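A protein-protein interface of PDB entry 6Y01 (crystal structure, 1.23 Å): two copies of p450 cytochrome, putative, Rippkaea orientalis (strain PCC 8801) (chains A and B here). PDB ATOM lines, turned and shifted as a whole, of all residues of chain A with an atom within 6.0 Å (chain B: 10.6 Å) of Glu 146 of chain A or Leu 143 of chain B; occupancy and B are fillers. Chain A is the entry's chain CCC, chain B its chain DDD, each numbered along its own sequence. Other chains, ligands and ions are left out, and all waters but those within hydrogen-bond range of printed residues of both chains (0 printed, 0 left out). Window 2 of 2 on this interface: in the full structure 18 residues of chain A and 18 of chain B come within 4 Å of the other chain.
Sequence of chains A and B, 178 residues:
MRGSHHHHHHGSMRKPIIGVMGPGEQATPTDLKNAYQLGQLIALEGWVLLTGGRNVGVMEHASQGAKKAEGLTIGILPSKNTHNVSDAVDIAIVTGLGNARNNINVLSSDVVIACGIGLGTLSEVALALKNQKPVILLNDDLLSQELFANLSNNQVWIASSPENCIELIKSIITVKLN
Among the printed residues, merely in contact across the chains: Asp 141 of chain A with Leu 147 of chain B, Leu 143 of chain A with Leu 143 of chain B, Leu 143 of chain A with Leu 147 of chain B, Leu 143 of chain A with Asn 150 of chain B, Glu 146 of chain A with Leu 143 of chain B, Leu 147 of chain A with Leu 122 of chain B, Leu 147 of chain A with Asp 141 of chain B, Leu 147 of chain A with Leu 143 of chain B, Leu 147 of chain A with Leu 147 of chain B, Phe 148 of chain A with Leu 122 of chain B, Asn 150 of chain A with Leu 143 of chain B and Leu 151 of chain A with Leu 119 of chain B.
The side-chain amide oxygen (OD1) of Asn 150 of chain A lies close to the backbone carbonyl oxygen (O) of Glu 146 of chain A (3.5 Å).
N of Leu 143 of chain A lies within hydrogen-bond range of OD1 of Asp 141 of chain A, 3.2 Å away.
OD1 of Asp 141 of chain A sits at hydrogen-bond distance from N of Ser 144 of chain A (2.9 Å).
The side-chain amide oxygen (OD1) of Asn 150 of chain B sits close to the backbone carbonyl oxygen (O) of Glu 146 of chain B, 3.4 Å away.
The side-chain carboxylate (OD2) of Asp 141 of chain B is in hydrogen-bond range of the side-chain hydroxyl (OG) of Ser 144 of chain B (2.8 Å).
The side-chain amide oxygen (OD1) of Asn 139 of chain B is in hydrogen-bond range of the backbone NH (N) of Asp 141 of chain B (2.9 Å).
Asp 141 of chain A touches Leu 147 of chain B, and with the chains exchanged Leu 147 of chain A touches Asp 141 of chain B.
Leu 143 of chain A touches its own counterpart, Leu 143 of chain B.
Leu 143 of chain A touches Leu 147 of chain B, and with the chains exchanged Leu 147 of chain A touches Leu 143 of chain B.
Glu 146 of chain A touches Leu 143 of chain B, but with the chains exchanged Leu 143 of chain A does not touch Glu 146 of chain B (4.1 Å).
Of the 12 pairs that touch across the chains among the printed residues, 8 have their exchanged pair printed and touching as well.
Printed residues of chain B within 4 Å of Asp 141 of chain A: Leu 147.
No residue of chain B comes within 4 Å of Ser 144 of chain A.
Glu 146 of chain A touches just one residue of chain B: Leu 143 (3.6 Å).
Printed residues of chain B within 4 Å of Phe 148 of chain A: Leu 122 (3.4 Å).
Of the printed residues of chain A, Leu 122 of chain B touches Leu 147 and Phe 148.
Leu 143 of chain B touches just these residues of chain A: Leu 143 (3.2 Å), Glu 146 (3.6 Å), Leu 147 (3.9 Å) and Asn 150 (3.8 Å).
Ser 144 of chain B touches none of the printed residues of chain A.
The nearest residue of chain A that does not touch Leu 143 of chain B is Leu 142 of chain A (5.9 Å).
The nearest printed residue of chain A that does not touch Leu 119 of chain B is Phe 148 of chain A (4.4 Å).
Hydrophobic or aromatic side chains of chain A that line the printed part of chain B: Leu 143, Leu 147, Phe 148 and Leu 151.
Along chain A the printed residues that touch a printed residue of chain B span positions 141 to 151.
Hydrophobic or aromatic side chains of chain B that line the printed part of chain A: Leu 119, Leu 122, Leu 143 and Leu 147.
Among the printed residues, 12 pairs touch across the chains.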
ATOM      1  N   ASP A 141       9.152 -29.625 -17.016  1.00  0.00           N
ATOM      2  CA  ASP A 141       9.345 -28.791 -18.223  1.00  0.00           C
ATOM      3  C   ASP A 141       9.622 -29.707 -19.408  1.00  0.00           C
ATOM      4  O   ASP A 141      10.795 -30.103 -19.635  1.00  0.00           O
ATOM      5  CB  ASP A 141      10.525 -27.831 -18.038  1.00  0.00           C
ATOM      6  CG  ASP A 141      10.621 -26.796 -19.138  1.00  0.00           C
ATOM      7  OD1 ASP A 141      10.675 -27.141 -20.278  1.00  0.00           O
ATOM      8  OD2 ASP A 141      10.598 -25.619 -18.833  1.00  0.00           O
ATOM      9  N   LEU A 142       8.604 -30.040 -20.167  1.00  0.00           N
ATOM     10  CA  LEU A 142       8.756 -30.994 -21.287  1.00  0.00           C
ATOM     11  C   LEU A 142       9.649 -30.400 -22.389  1.00  0.00           C
ATOM     12  O   LEU A 142      10.339 -31.182 -23.035  1.00  0.00           O
ATOM     13  CB  LEU A 142       7.376 -31.356 -21.827  1.00  0.00           C
ATOM     14  CG  LEU A 142       6.426 -32.042 -20.856  1.00  0.00           C
ATOM     15  CD1 LEU A 142       5.159 -32.387 -21.606  1.00  0.00           C
ATOM     16  CD2 LEU A 142       7.035 -33.294 -20.236  1.00  0.00           C
ATOM     17  N   LEU A 143       9.684 -29.074 -22.564  1.00  0.00           N
ATOM     18  CA  LEU A 143      10.572 -28.429 -23.569  1.00  0.00           C
ATOM     19  C   LEU A 143      12.035 -28.762 -23.263  1.00  0.00           C
ATOM     20  O   LEU A 143      12.746 -29.206 -24.183  1.00  0.00           O
ATOM     21  CB  LEU A 143      10.439 -26.904 -23.557  1.00  0.00           C
ATOM     22  CG  LEU A 143       9.281 -26.283 -24.304  1.00  0.00           C
ATOM     23  CD1 LEU A 143       9.312 -24.771 -24.104  1.00  0.00           C
ATOM     24  CD2 LEU A 143       9.353 -26.640 -25.767  1.00  0.00           C
ATOM     25  N   SER A 144      12.485 -28.527 -22.034  1.00  0.00           N
ATOM     26  CA  SER A 144      13.869 -28.795 -21.600  1.00  0.00           C
ATOM     27  C   SER A 144      14.183 -30.279 -21.740  1.00  0.00           C
ATOM     28  O   SER A 144      15.291 -30.622 -22.136  1.00  0.00           O
ATOM     29  CB  SER A 144      14.139 -28.293 -20.165  1.00  0.00           C
ATOM     30  OG  SER A 144      13.491 -29.113 -19.161  1.00  0.00           O
ATOM     31  N   GLN A 145      13.223 -31.149 -21.424  1.00  0.00           N
ATOM     32  CA  GLN A 145      13.442 -32.603 -21.441  1.00  0.00           C
ATOM     33  C   GLN A 145      13.676 -33.010 -22.901  1.00  0.00           C
ATOM     34  O   GLN A 145      14.685 -33.700 -23.168  1.00  0.00           O
ATOM     35  CB  GLN A 145      12.240 -33.336 -20.853  1.00  0.00           C
ATOM     36  CG  GLN A 145      12.085 -33.137 -19.357  1.00  0.00           C
ATOM     37  CD  GLN A 145      10.811 -33.759 -18.832  1.00  0.00           C
ATOM     38  OE1 GLN A 145      10.273 -34.653 -19.454  1.00  0.00           O
ATOM     39  NE2 GLN A 145      10.379 -33.307 -17.651  1.00  0.00           N
ATOM     40  N   GLU A 146      12.844 -32.535 -23.827  1.00  0.00           N
ATOM     41  CA  GLU A 146      12.982 -32.910 -25.233  1.00  0.00           C
ATOM     42  C   GLU A 146      14.277 -32.287 -25.793  1.00  0.00           C
ATOM     43  O   GLU A 146      15.022 -32.972 -26.500  1.00  0.00           O
ATOM     44  CB  GLU A 146      11.775 -32.430 -26.020  1.00  0.00           C
ATOM     45  CG  GLU A 146      11.763 -33.033 -27.421  1.00  0.00           C
ATOM     46  CD  GLU A 146      10.653 -32.535 -28.324  1.00  0.00           C
ATOM     47  OE1 GLU A 146       9.752 -31.806 -27.831  1.00  0.00           O
ATOM     48  OE2 GLU A 146      10.713 -32.854 -29.547  1.00  0.00           O
ATOM     49  N   LEU A 147      14.554 -31.032 -25.493  1.00  0.00           N
ATOM     50  CA  LEU A 147      15.768 -30.361 -25.992  1.00  0.00           C
ATOM     51  C   LEU A 147      17.030 -31.102 -25.550  1.00  0.00           C
ATOM     52  O   LEU A 147      17.890 -31.386 -26.364  1.00  0.00           O
ATOM     53  CB  LEU A 147      15.794 -28.920 -25.485  1.00  0.00           C
ATOM     54  CG  LEU A 147      17.013 -28.098 -25.890  1.00  0.00           C
ATOM     55  CD1 LEU A 147      17.128 -28.007 -27.407  1.00  0.00           C
ATOM     56  CD2 LEU A 147      16.914 -26.745 -25.209  1.00  0.00           C
ATOM     57  N   PHE A 148      17.133 -31.464 -24.276  1.00  0.00           N
ATOM     58  CA  PHE A 148      18.339 -32.138 -23.802  1.00  0.00           C
ATOM     59  C   PHE A 148      18.400 -33.566 -24.284  1.00  0.00           C
ATOM     60  O   PHE A 148      19.513 -34.043 -24.501  1.00  0.00           O
ATOM     61  CB  PHE A 148      18.492 -32.020 -22.296  1.00  0.00           C
ATOM     62  CG  PHE A 148      18.905 -30.641 -21.875  1.00  0.00           C
ATOM     63  CD1 PHE A 148      20.074 -30.102 -22.338  1.00  0.00           C
ATOM     64  CD2 PHE A 148      18.182 -29.946 -20.909  1.00  0.00           C
ATOM     65  CE1 PHE A 148      20.510 -28.871 -21.900  1.00  0.00           C
ATOM     66  CE2 PHE A 148      18.589 -28.696 -20.509  1.00  0.00           C
ATOM     67  CZ  PHE A 148      19.752 -28.156 -21.008  1.00  0.00           C
ATOM     68  N   ALA A 149      17.260 -34.255 -24.443  1.00  0.00           N
ATOM     69  CA  ALA A 149      17.269 -35.607 -25.034  1.00  0.00           C
ATOM     70  C   ALA A 149      17.852 -35.487 -26.446  1.00  0.00           C
ATOM     71  O   ALA A 149      18.722 -36.279 -26.841  1.00  0.00           O
ATOM     72  CB  ALA A 149      15.872 -36.182 -25.091  1.00  0.00           C
ATOM     73  N   ASN A 150      17.424 -34.492 -27.195  1.00  0.00           N
ATOM     74  CA  ASN A 150      17.892 -34.312 -28.598  1.00  0.00           C
ATOM     75  C   ASN A 150      19.390 -34.005 -28.629  1.00  0.00           C
ATOM     76  O   ASN A 150      20.130 -34.684 -29.359  1.00  0.00           O
ATOM     77  CB  ASN A 150      17.122 -33.205 -29.319  1.00  0.00           C
ATOM     78  CG  ASN A 150      15.681 -33.573 -29.605  1.00  0.00           C
ATOM     79  OD1 ASN A 150      15.307 -34.730 -29.501  1.00  0.00           O
ATOM     80  ND2 ASN A 150      14.872 -32.604 -30.002  1.00  0.00           N
ATOM     81  N   LEU A 151      19.832 -33.047 -27.830  1.00  0.00           N
ATOM     82  CA  LEU A 151      21.237 -32.578 -27.880  1.00  0.00           C
ATOM     83  C   LEU A 151      22.184 -33.588 -27.263  1.00  0.00           C
ATOM     84  O   LEU A 151      23.381 -33.486 -27.538  1.00  0.00           O
ATOM     85  CB  LEU A 151      21.376 -31.220 -27.207  1.00  0.00           C
ATOM     86  CG  LEU A 151      20.752 -30.066 -27.981  1.00  0.00           C
ATOM     87  CD1 LEU A 151      20.921 -28.789 -27.197  1.00  0.00           C
ATOM     88  CD2 LEU A 151      21.303 -29.939 -29.401  1.00  0.00           C
ATOM     89  N   ILE B 117      22.827 -24.067 -32.974  1.00  0.00           N
ATOM     90  CA  ILE B 117      22.575 -24.542 -31.585  1.00  0.00           C
ATOM     91  C   ILE B 117      23.393 -25.791 -31.346  1.00  0.00           C
ATOM     92  O   ILE B 117      23.711 -26.551 -32.253  1.00  0.00           O
ATOM     93  CB  ILE B 117      21.072 -24.766 -31.380  1.00  0.00           C
ATOM     94  CG1 ILE B 117      20.749 -24.883 -29.892  1.00  0.00           C
ATOM     95  CG2 ILE B 117      20.645 -25.977 -32.170  1.00  0.00           C
ATOM     96  CD1 ILE B 117      20.891 -23.544 -29.166  1.00  0.00           C
ATOM     97  N   LEU B 119      25.300 -27.826 -27.406  1.00  0.00           N
ATOM     98  CA  LEU B 119      25.371 -27.749 -25.948  1.00  0.00           C
ATOM     99  C   LEU B 119      26.146 -26.516 -25.483  1.00  0.00           C
ATOM    100  O   LEU B 119      25.718 -25.810 -24.556  1.00  0.00           O
ATOM    101  CB  LEU B 119      25.958 -29.046 -25.434  1.00  0.00           C
ATOM    102  CG  LEU B 119      25.034 -30.259 -25.558  1.00  0.00           C
ATOM    103  CD1 LEU B 119      25.799 -31.537 -25.260  1.00  0.00           C
ATOM    104  CD2 LEU B 119      23.873 -30.140 -24.530  1.00  0.00           C
ATOM    105  N   LEU B 122      24.114 -23.427 -26.090  1.00  0.00           N
ATOM    106  CA  LEU B 122      22.990 -23.340 -25.113  1.00  0.00           C
ATOM    107  C   LEU B 122      23.491 -22.761 -23.797  1.00  0.00           C
ATOM    108  O   LEU B 122      22.810 -21.874 -23.212  1.00  0.00           O
ATOM    109  CB  LEU B 122      22.411 -24.724 -24.877  1.00  0.00           C
ATOM    110  CG  LEU B 122      21.004 -24.769 -24.348  1.00  0.00           C
ATOM    111  CD1 LEU B 122      20.000 -24.299 -25.397  1.00  0.00           C
ATOM    112  CD2 LEU B 122      20.687 -26.208 -24.000  1.00  0.00           C
ATOM    113  N   VAL B 125      24.110 -18.929 -24.302  1.00  0.00           N
ATOM    114  CA  VAL B 125      22.836 -18.172 -24.373  1.00  0.00           C
ATOM    115  C   VAL B 125      22.224 -18.068 -22.973  1.00  0.00           C
ATOM    116  O   VAL B 125      21.794 -16.998 -22.616  1.00  0.00           O
ATOM    117  CB  VAL B 125      21.874 -18.809 -25.356  1.00  0.00           C
ATOM    118  CG1 VAL B 125      20.491 -18.199 -25.271  1.00  0.00           C
ATOM    119  CG2 VAL B 125      22.406 -18.690 -26.791  1.00  0.00           C
ATOM    120  N   LEU B 129      21.561 -14.528 -21.090  1.00  0.00           N
ATOM    121  CA  LEU B 129      20.219 -14.085 -20.628  1.00  0.00           C
ATOM    122  C   LEU B 129      20.189 -13.927 -19.102  1.00  0.00           C
ATOM    123  O   LEU B 129      19.584 -12.986 -18.647  1.00  0.00           O
ATOM    124  CB  LEU B 129      19.201 -15.114 -21.096  1.00  0.00           C
ATOM    125  CG  LEU B 129      18.958 -15.147 -22.603  1.00  0.00           C
ATOM    126  CD1 LEU B 129      18.100 -16.325 -22.976  1.00  0.00           C
ATOM    127  CD2 LEU B 129      18.337 -13.864 -23.091  1.00  0.00           C
ATOM    128  N   LEU B 137      18.969 -14.985 -31.500  1.00  0.00           N
ATOM    129  CA  LEU B 137      19.056 -16.368 -31.994  1.00  0.00           C
ATOM    130  C   LEU B 137      18.891 -16.371 -33.507  1.00  0.00           C
ATOM    131  O   LEU B 137      17.914 -15.857 -34.022  1.00  0.00           O
ATOM    132  CB  LEU B 137      17.974 -17.220 -31.333  1.00  0.00           C
ATOM    133  CG  LEU B 137      17.970 -17.190 -29.798  1.00  0.00           C
ATOM    134  CD1 LEU B 137      16.818 -18.066 -29.276  1.00  0.00           C
ATOM    135  CD2 LEU B 137      19.279 -17.659 -29.242  1.00  0.00           C
ATOM    136  N   ASN B 139      18.787 -19.442 -35.827  1.00  0.00           N
ATOM    137  CA  ASN B 139      18.807 -20.908 -35.906  1.00  0.00           C
ATOM    138  C   ASN B 139      17.451 -21.415 -36.337  1.00  0.00           C
ATOM    139  O   ASN B 139      16.502 -20.621 -36.428  1.00  0.00           O
ATOM    140  CB  ASN B 139      19.237 -21.564 -34.592  1.00  0.00           C
ATOM    141  CG  ASN B 139      18.265 -21.393 -33.456  1.00  0.00           C
ATOM    142  OD1 ASN B 139      17.053 -21.586 -33.620  1.00  0.00           O
ATOM    143  ND2 ASN B 139      18.810 -20.968 -32.338  1.00  0.00           N
ATOM    144  N   ASP B 140      17.400 -22.715 -36.580  1.00  0.00           N
ATOM    145  CA  ASP B 140      16.172 -23.407 -37.022  1.00  0.00           C
ATOM    146  C   ASP B 140      15.701 -24.363 -35.932  1.00  0.00           C
ATOM    147  O   ASP B 140      15.177 -25.408 -36.287  1.00  0.00           O
ATOM    148  CB  ASP B 140      16.416 -24.126 -38.350  1.00  0.00           C
ATOM    149  CG  ASP B 140      16.661 -23.142 -39.474  1.00  0.00           C
ATOM    150  OD1 ASP B 140      15.925 -22.121 -39.514  1.00  0.00           O
ATOM    151  OD2 ASP B 140      17.615 -23.366 -40.279  1.00  0.00           O
ATOM    152  N   ASP B 141      15.901 -23.995 -34.662  1.00  0.00           N
ATOM    153  CA  ASP B 141      15.539 -24.839 -33.502  1.00  0.00           C
ATOM    154  C   ASP B 141      14.396 -24.183 -32.717  1.00  0.00           C
ATOM    155  O   ASP B 141      14.652 -23.398 -31.791  1.00  0.00           O
ATOM    156  CB  ASP B 141      16.742 -25.083 -32.591  1.00  0.00           C
ATOM    157  CG  ASP B 141      16.466 -26.138 -31.540  1.00  0.00           C
ATOM    158  OD1 ASP B 141      16.198 -27.252 -31.917  1.00  0.00           O
ATOM    159  OD2 ASP B 141      16.443 -25.791 -30.332  1.00  0.00           O
ATOM    160  N   LEU B 142      13.162 -24.557 -33.036  1.00  0.00           N
ATOM    161  CA  LEU B 142      11.974 -23.951 -32.406  1.00  0.00           C
ATOM    162  C   LEU B 142      11.910 -24.271 -30.910  1.00  0.00           C
ATOM    163  O   LEU B 142      11.436 -23.408 -30.163  1.00  0.00           O
ATOM    164  CB  LEU B 142      10.724 -24.422 -33.141  1.00  0.00           C
ATOM    165  CG  LEU B 142      10.634 -24.010 -34.601  1.00  0.00           C
ATOM    166  CD1 LEU B 142       9.362 -24.588 -35.201  1.00  0.00           C
ATOM    167  CD2 LEU B 142      10.690 -22.483 -34.742  1.00  0.00           C
ATOM    168  N   LEU B 143      12.399 -25.437 -30.475  1.00  0.00           N
ATOM    169  CA  LEU B 143      12.393 -25.811 -29.036  1.00  0.00           C
ATOM    170  C   LEU B 143      13.223 -24.807 -28.239  1.00  0.00           C
ATOM    171  O   LEU B 143      12.722 -24.303 -27.208  1.00  0.00           O
ATOM    172  CB  LEU B 143      12.977 -27.205 -28.798  1.00  0.00           C
ATOM    173  CG  LEU B 143      12.075 -28.406 -28.992  1.00  0.00           C
ATOM    174  CD1 LEU B 143      12.869 -29.670 -28.680  1.00  0.00           C
ATOM    175  CD2 LEU B 143      10.863 -28.305 -28.111  1.00  0.00           C
ATOM    176  N   SER B 144      14.472 -24.568 -28.658  1.00  0.00           N
ATOM    177  CA  SER B 144      15.375 -23.624 -27.960  1.00  0.00           C
ATOM    178  C   SER B 144      14.769 -22.222 -27.978  1.00  0.00           C
ATOM    179  O   SER B 144      14.884 -21.529 -26.968  1.00  0.00           O
ATOM    180  CB  SER B 144      16.809 -23.628 -28.518  1.00  0.00           C
ATOM    181  OG  SER B 144      16.880 -23.075 -29.829  1.00  0.00           O
ATOM    182  N   GLN B 145      14.117 -21.834 -29.068  1.00  0.00           N
ATOM    183  CA  GLN B 145      13.554 -20.479 -29.205  1.00  0.00           C
ATOM    184  C   GLN B 145      12.446 -20.306 -28.170  1.00  0.00           C
ATOM    185  O   GLN B 145      12.465 -19.324 -27.420  1.00  0.00           O
ATOM    186  CB  GLN B 145      13.077 -20.216 -30.636  1.00  0.00           C
ATOM    187  CG  GLN B 145      14.225 -20.172 -31.645  1.00  0.00           C
ATOM    188  CD  GLN B 145      13.728 -19.986 -33.060  1.00  0.00           C
ATOM    189  OE1 GLN B 145      12.584 -19.601 -33.282  1.00  0.00           O
ATOM    190  NE2 GLN B 145      14.587 -20.295 -34.027  1.00  0.00           N
ATOM    191  N   GLU B 146      11.552 -21.279 -28.093  1.00  0.00           N
ATOM    192  CA  GLU B 146      10.416 -21.235 -27.135  1.00  0.00           C
ATOM    193  C   GLU B 146      10.958 -21.273 -25.696  1.00  0.00           C
ATOM    194  O   GLU B 146      10.529 -20.477 -24.846  1.00  0.00           O
ATOM    195  CB  GLU B 146       9.476 -22.409 -27.391  1.00  0.00           C
ATOM    196  N   LEU B 147      11.898 -22.167 -25.419  1.00  0.00           N
ATOM    197  CA  LEU B 147      12.431 -22.302 -24.049  1.00  0.00           C
ATOM    198  C   LEU B 147      13.067 -20.986 -23.584  1.00  0.00           C
ATOM    199  O   LEU B 147      12.776 -20.505 -22.476  1.00  0.00           O
ATOM    200  CB  LEU B 147      13.446 -23.437 -24.016  1.00  0.00           C
ATOM    201  CG  LEU B 147      14.028 -23.724 -22.630  1.00  0.00           C
ATOM    202  CD1 LEU B 147      12.953 -23.967 -21.553  1.00  0.00           C
ATOM    203  CD2 LEU B 147      14.914 -24.951 -22.714  1.00  0.00           C
ATOM    204  N   PHE B 148      13.917 -20.387 -24.418  1.00  0.00           N
ATOM    205  CA  PHE B 148      14.593 -19.138 -24.027  1.00  0.00           C
ATOM    206  C   PHE B 148      13.606 -17.966 -23.942  1.00  0.00           C
ATOM    207  O   PHE B 148      13.799 -17.102 -23.090  1.00  0.00           O
ATOM    208  CB  PHE B 148      15.764 -18.859 -24.968  1.00  0.00           C
ATOM    209  CG  PHE B 148      16.943 -19.729 -24.673  1.00  0.00           C
ATOM    210  CD1 PHE B 148      17.463 -19.815 -23.389  1.00  0.00           C
ATOM    211  CD2 PHE B 148      17.563 -20.441 -25.679  1.00  0.00           C
ATOM    212  CE1 PHE B 148      18.557 -20.588 -23.108  1.00  0.00           C
ATOM    213  CE2 PHE B 148      18.671 -21.220 -25.412  1.00  0.00           C
ATOM    214  CZ  PHE B 148      19.172 -21.278 -24.127  1.00  0.00           C
ATOM    215  N   ALA B 149      12.600 -17.917 -24.807  1.00  0.00           N
ATOM    216  CA  ALA B 149      11.572 -16.860 -24.736  1.00  0.00           C
ATOM    217  C   ALA B 149      10.873 -16.980 -23.372  1.00  0.00           C
ATOM    218  O   ALA B 149      10.689 -15.977 -22.689  1.00  0.00           O
ATOM    219  CB  ALA B 149      10.582 -16.978 -25.879  1.00  0.00           C
ATOM    220  N   ASN B 150      10.554 -18.201 -22.958  1.00  0.00           N
ATOM    221  CA  ASN B 150       9.846 -18.422 -21.674  1.00  0.00           C
ATOM    222  C   ASN B 150      10.742 -17.996 -20.495  1.00  0.00           C
ATOM    223  O   ASN B 150      10.291 -17.206 -19.643  1.00  0.00           O
ATOM    224  CB  ASN B 150       9.437 -19.879 -21.501  1.00  0.00           C
ATOM    225  CG  ASN B 150       8.362 -20.331 -22.460  1.00  0.00           C
ATOM    226  OD1 ASN B 150       7.727 -19.515 -23.130  1.00  0.00           O
ATOM    227  ND2 ASN B 150       8.141 -21.638 -22.521  1.00  0.00           N
ATOM    228  N   LEU B 151      11.989 -18.459 -20.475  1.00  0.00           N
ATOM    229  CA  LEU B 151      12.889 -18.223 -19.327  1.00  0.00           C
ATOM    230  C   LEU B 151      13.359 -16.779 -19.272  1.00  0.00           C
ATOM    231  O   LEU B 151      13.788 -16.349 -18.187  1.00  0.00           O
ATOM    232  CB  LEU B 151      14.084 -19.170 -19.371  1.00  0.00           C
ATOM    233  CG  LEU B 151      13.736 -20.630 -19.079  1.00  0.00           C
ATOM    234  CD1 LEU B 151      14.948 -21.496 -19.216  1.00  0.00           C
ATOM    235  CD2 LEU B 151      13.078 -20.809 -17.717  1.00  0.00           C
ATOM    236  N   VAL B 156      14.749 -12.322 -25.302  1.00  0.00           N
ATOM    237  CA  VAL B 156      15.545 -12.846 -26.424  1.00  0.00           C
ATOM    238  C   VAL B 156      14.933 -12.403 -27.762  1.00  0.00           C
ATOM    239  O   VAL B 156      13.730 -12.291 -27.901  1.00  0.00           O
ATOM    240  CB  VAL B 156      15.635 -14.367 -26.276  1.00  0.00           C
ATOM    241  CG1 VAL B 156      14.326 -15.047 -26.591  1.00  0.00           C
ATOM    242  CG2 VAL B 156      16.734 -14.920 -27.121  1.00  0.00           C
ATOM    243  N   ILE B 158      14.722 -13.171 -32.012  1.00  0.00           N
ATOM    244  CA  ILE B 158      14.829 -14.218 -33.046  1.00  0.00           C
ATOM    245  C   ILE B 158      15.068 -13.527 -34.390  1.00  0.00           C
ATOM    246  O   ILE B 158      14.221 -12.771 -34.832  1.00  0.00           O
ATOM    247  CB  ILE B 158      13.568 -15.089 -33.121  1.00  0.00           C
ATOM    248  CG1 ILE B 158      13.152 -15.580 -31.734  1.00  0.00           C
ATOM    249  CG2 ILE B 158      13.798 -16.233 -34.099  1.00  0.00           C
ATOM    250  CD1 ILE B 158      14.130 -16.450 -31.068  1.00  0.00           C
